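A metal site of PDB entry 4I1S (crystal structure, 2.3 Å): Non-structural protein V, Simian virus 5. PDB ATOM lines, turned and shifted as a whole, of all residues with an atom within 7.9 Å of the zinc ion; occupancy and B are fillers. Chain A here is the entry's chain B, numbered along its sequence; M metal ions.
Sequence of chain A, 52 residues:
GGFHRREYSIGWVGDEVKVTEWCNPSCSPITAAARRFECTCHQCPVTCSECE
Within 4 Å of the zinc ion: His 4, Cys 23, Cys 48 and Cys 51.
The zinc ion is bound by ND1 of His 4, SG of Cys 51, SG of Cys 48 and SG of Cys 23. The zinc ion has four donor atoms within binding distance.
NE2 of His 4 is in hydrogen-bond range of O of Pro 45 (3.2 Å). The backbone NH (N) of Glu 50 lies close to the side-chain sulfur (SG) of Cys 48 (3.5 Å). The side-chain sulfur (SG) of Cys 23 sits close to the guanidinium group (NH1) of Arg 6.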
ATOM      1  N   PHE A   3     -27.639  13.810  18.866  1.00  0.00           N
ATOM      2  CA  PHE A   3     -28.162  12.764  19.748  1.00  0.00           C
ATOM      3  C   PHE A   3     -27.492  12.732  21.138  1.00  0.00           C
ATOM      4  O   PHE A   3     -26.722  13.619  21.493  1.00  0.00           O
ATOM      5  CB  PHE A   3     -28.090  11.397  19.066  1.00  0.00           C
ATOM      6  CG  PHE A   3     -26.683  10.982  18.668  1.00  0.00           C
ATOM      7  CD1 PHE A   3     -26.126  11.433  17.470  1.00  0.00           C
ATOM      8  CD2 PHE A   3     -25.937  10.147  19.487  1.00  0.00           C
ATOM      9  CE1 PHE A   3     -24.830  11.066  17.103  1.00  0.00           C
ATOM     10  CE2 PHE A   3     -24.636   9.777  19.128  1.00  0.00           C
ATOM     11  CZ  PHE A   3     -24.078  10.236  17.933  1.00  0.00           C
ATOM     12  N   HIS A   4     -27.819  11.718  21.925  1.00  0.00           N
ATOM     13  CA  HIS A   4     -27.183  11.519  23.227  1.00  0.00           C
ATOM     14  C   HIS A   4     -26.130  10.424  23.156  1.00  0.00           C
ATOM     15  O   HIS A   4     -26.402   9.307  22.706  1.00  0.00           O
ATOM     16  CB  HIS A   4     -28.183  11.113  24.316  1.00  0.00           C
ATOM     17  CG  HIS A   4     -28.849  12.275  24.992  1.00  0.00           C
ATOM     18  ND1 HIS A   4     -29.657  12.110  26.089  1.00  0.00           N
ATOM     19  CD2 HIS A   4     -28.830  13.600  24.730  1.00  0.00           C
ATOM     20  CE1 HIS A   4     -30.118  13.294  26.477  1.00  0.00           C
ATOM     21  NE2 HIS A   4     -29.634  14.210  25.661  1.00  0.00           N
ATOM     22  N   ARG A   5     -24.943  10.777  23.629  1.00  0.00           N
ATOM     23  CA  ARG A   5     -23.855   9.828  23.830  1.00  0.00           C
ATOM     24  C   ARG A   5     -23.904   9.324  25.270  1.00  0.00           C
ATOM     25  O   ARG A   5     -23.853  10.107  26.219  1.00  0.00           O
ATOM     26  CB  ARG A   5     -22.500  10.495  23.552  1.00  0.00           C
ATOM     27  CG  ARG A   5     -21.326   9.537  23.608  1.00  0.00           C
ATOM     28  CD  ARG A   5     -20.032  10.257  23.277  1.00  0.00           C
ATOM     29  NE  ARG A   5     -19.658  11.247  24.296  1.00  0.00           N
ATOM     30  CZ  ARG A   5     -19.563  12.555  24.073  1.00  0.00           C
ATOM     31  NH1 ARG A   5     -19.809  13.056  22.853  1.00  0.00           N
ATOM     32  NH2 ARG A   5     -19.210  13.368  25.054  1.00  0.00           N
ATOM     33  N   ARG A   6     -24.037   8.011  25.412  1.00  0.00           N
ATOM     34  CA  ARG A   6     -24.121   7.371  26.719  1.00  0.00           C
ATOM     35  C   ARG A   6     -22.716   7.280  27.320  1.00  0.00           C
ATOM     36  O   ARG A   6     -21.745   6.963  26.628  1.00  0.00           O
ATOM     37  CB  ARG A   6     -24.783   5.995  26.562  1.00  0.00           C
ATOM     38  CG  ARG A   6     -25.449   5.428  27.820  1.00  0.00           C
ATOM     39  CD  ARG A   6     -26.484   6.349  28.444  1.00  0.00           C
ATOM     40  NE  ARG A   6     -27.015   5.781  29.683  1.00  0.00           N
ATOM     41  CZ  ARG A   6     -27.686   6.475  30.599  1.00  0.00           C
ATOM     42  NH1 ARG A   6     -27.926   7.773  30.443  1.00  0.00           N
ATOM     43  NH2 ARG A   6     -28.127   5.863  31.698  1.00  0.00           N
ATOM     44  N   TRP A  22     -24.501   8.246  32.624  1.00  0.00           N
ATOM     45  CA  TRP A  22     -25.198   9.488  32.342  1.00  0.00           C
ATOM     46  C   TRP A  22     -25.159   9.737  30.833  1.00  0.00           C
ATOM     47  O   TRP A  22     -24.729   8.875  30.067  1.00  0.00           O
ATOM     48  CB  TRP A  22     -24.571  10.648  33.120  1.00  0.00           C
ATOM     49  CG  TRP A  22     -23.178  11.057  32.687  1.00  0.00           C
ATOM     50  CD1 TRP A  22     -22.850  12.142  31.910  1.00  0.00           C
ATOM     51  CD2 TRP A  22     -21.940  10.422  33.024  1.00  0.00           C
ATOM     52  NE1 TRP A  22     -21.486  12.203  31.726  1.00  0.00           N
ATOM     53  CE2 TRP A  22     -20.908  11.155  32.405  1.00  0.00           C
ATOM     54  CE3 TRP A  22     -21.610   9.293  33.778  1.00  0.00           C
ATOM     55  CZ2 TRP A  22     -19.573  10.797  32.510  1.00  0.00           C
ATOM     56  CZ3 TRP A  22     -20.274   8.944  33.887  1.00  0.00           C
ATOM     57  CH2 TRP A  22     -19.278   9.684  33.264  1.00  0.00           C
ATOM     58  N   CYS A  23     -25.588  10.910  30.407  1.00  0.00           N
ATOM     59  CA  CYS A  23     -25.641  11.233  28.992  1.00  0.00           C
ATOM     60  C   CYS A  23     -24.941  12.551  28.688  1.00  0.00           C
ATOM     61  O   CYS A  23     -25.032  13.516  29.454  1.00  0.00           O
ATOM     62  CB  CYS A  23     -27.096  11.324  28.515  1.00  0.00           C
ATOM     63  SG  CYS A  23     -27.849   9.752  28.150  1.00  0.00           S
ATOM     64  N   ASN A  24     -24.261  12.581  27.542  1.00  0.00           N
ATOM     65  CA  ASN A  24     -23.687  13.812  27.016  1.00  0.00           C
ATOM     66  C   ASN A  24     -24.320  14.108  25.661  1.00  0.00           C
ATOM     67  O   ASN A  24     -24.773  13.181  24.968  1.00  0.00           O
ATOM     68  CB  ASN A  24     -22.174  13.704  26.871  1.00  0.00           C
ATOM     69  CG  ASN A  24     -21.429  14.205  28.101  1.00  0.00           C
ATOM     70  OD1 ASN A  24     -21.900  15.107  28.785  1.00  0.00           O
ATOM     71  ND2 ASN A  24     -20.276  13.617  28.382  1.00  0.00           N
ATOM     72  N   PRO A  25     -24.367  15.393  25.279  1.00  0.00           N
ATOM     73  CA  PRO A  25     -24.801  15.756  23.929  1.00  0.00           C
ATOM     74  C   PRO A  25     -23.762  15.252  22.919  1.00  0.00           C
ATOM     75  O   PRO A  25     -22.569  15.309  23.234  1.00  0.00           O
ATOM     76  CB  PRO A  25     -24.811  17.285  23.951  1.00  0.00           C
ATOM     77  CG  PRO A  25     -24.733  17.664  25.399  1.00  0.00           C
ATOM     78  CD  PRO A  25     -24.003  16.568  26.088  1.00  0.00           C
ATOM     79  N   PRO A  45     -31.171  16.759  21.641  1.00  0.00           N
ATOM     80  CA  PRO A  45     -32.369  16.654  22.488  1.00  0.00           C
ATOM     81  C   PRO A  45     -32.079  16.869  23.969  1.00  0.00           C
ATOM     82  O   PRO A  45     -30.919  16.802  24.388  1.00  0.00           O
ATOM     83  CB  PRO A  45     -32.847  15.221  22.247  1.00  0.00           C
ATOM     84  CG  PRO A  45     -31.642  14.476  21.743  1.00  0.00           C
ATOM     85  CD  PRO A  45     -30.881  15.499  20.937  1.00  0.00           C
ATOM     86  N   VAL A  46     -33.116  17.119  24.771  1.00  0.00           N
ATOM     87  CA  VAL A  46     -32.918  17.358  26.201  1.00  0.00           C
ATOM     88  C   VAL A  46     -32.794  16.046  26.970  1.00  0.00           C
ATOM     89  O   VAL A  46     -31.998  15.953  27.901  1.00  0.00           O
ATOM     90  CB  VAL A  46     -34.063  18.199  26.794  1.00  0.00           C
ATOM     91  CG1 VAL A  46     -33.544  19.586  27.162  1.00  0.00           C
ATOM     92  CG2 VAL A  46     -35.209  18.290  25.806  1.00  0.00           C
ATOM     93  N   THR A  47     -33.597  15.058  26.607  1.00  0.00           N
ATOM     94  CA  THR A  47     -33.503  13.724  27.198  1.00  0.00           C
ATOM     95  C   THR A  47     -33.634  12.636  26.118  1.00  0.00           C
ATOM     96  O   THR A  47     -34.178  12.884  25.037  1.00  0.00           O
ATOM     97  CB  THR A  47     -34.576  13.478  28.267  1.00  0.00           C
ATOM     98  OG1 THR A  47     -35.847  13.290  27.635  1.00  0.00           O
ATOM     99  CG2 THR A  47     -34.658  14.635  29.255  1.00  0.00           C
ATOM    100  N   CYS A  48     -33.143  11.440  26.417  1.00  0.00           N
ATOM    101  CA  CYS A  48     -33.405  10.288  25.568  1.00  0.00           C
ATOM    102  C   CYS A  48     -34.044   9.165  26.386  1.00  0.00           C
ATOM    103  O   CYS A  48     -34.304   9.330  27.572  1.00  0.00           O
ATOM    104  CB  CYS A  48     -32.122   9.802  24.882  1.00  0.00           C
ATOM    105  SG  CYS A  48     -30.813   9.211  25.996  1.00  0.00           S
ATOM    106  N   SER A  49     -34.300   8.029  25.737  1.00  0.00           N
ATOM    107  CA  SER A  49     -34.873   6.880  26.436  1.00  0.00           C
ATOM    108  C   SER A  49     -33.999   6.459  27.609  1.00  0.00           C
ATOM    109  O   SER A  49     -34.501   6.003  28.643  1.00  0.00           O
ATOM    110  CB  SER A  49     -35.000   5.710  25.474  1.00  0.00           C
ATOM    111  OG  SER A  49     -33.774   5.020  25.364  1.00  0.00           O
ATOM    112  N   GLU A  50     -32.690   6.643  27.464  1.00  0.00           N
ATOM    113  CA  GLU A  50     -31.715   6.196  28.451  1.00  0.00           C
ATOM    114  C   GLU A  50     -31.643   7.058  29.707  1.00  0.00           C
ATOM    115  O   GLU A  50     -31.323   6.562  30.782  1.00  0.00           O
ATOM    116  CB  GLU A  50     -30.324   6.065  27.820  1.00  0.00           C
ATOM    117  CG  GLU A  50     -30.206   4.863  26.902  1.00  0.00           C
ATOM    118  CD  GLU A  50     -30.782   3.608  27.515  1.00  0.00           C
ATOM    119  OE1 GLU A  50     -30.069   2.963  28.307  1.00  0.00           O
ATOM    120  OE2 GLU A  50     -31.958   3.275  27.229  1.00  0.00           O
ATOM    121  N   CYS A  51     -31.925   8.340  29.577  1.00  0.00           N
ATOM    122  CA  CYS A  51     -31.952   9.210  30.741  1.00  0.00           C
ATOM    123  C   CYS A  51     -33.371   9.684  31.051  1.00  0.00           C
ATOM    124  O   CYS A  51     -33.575  10.777  31.570  1.00  0.00           O
ATOM    125  CB  CYS A  51     -30.980  10.389  30.574  1.00  0.00           C
ATOM    126  SG  CYS A  51     -31.251  11.400  29.100  1.00  0.00           S
ATOM    127  N   GLU A  52     -34.341   8.817  30.745  1.00  0.00           N
ATOM    128  CA  GLU A  52     -35.782   9.093  30.825  1.00  0.00           C
ATOM    129  C   GLU A  52     -36.262  10.039  29.718  1.00  0.00           C
ATOM    130  O   GLU A  52     -37.181   9.704  28.972  1.00  0.00           O
ATOM    131  CB  GLU A  52     -36.204   9.630  32.199  1.00  0.00           C
ATOM    132  CG  GLU A  52     -35.822   8.751  33.363  1.00  0.00           C
ATOM    133  CD  GLU A  52     -36.199   9.393  34.679  1.00  0.00           C
ATOM    134  OE1 GLU A  52     -36.615  10.575  34.629  1.00  0.00           O
ATOM    135  OE2 GLU A  52     -36.092   8.730  35.733  1.00  0.00           O
HETATM  136 ZN    ZN M   1     -29.981  10.711  27.420  1.00  0.00          ZN
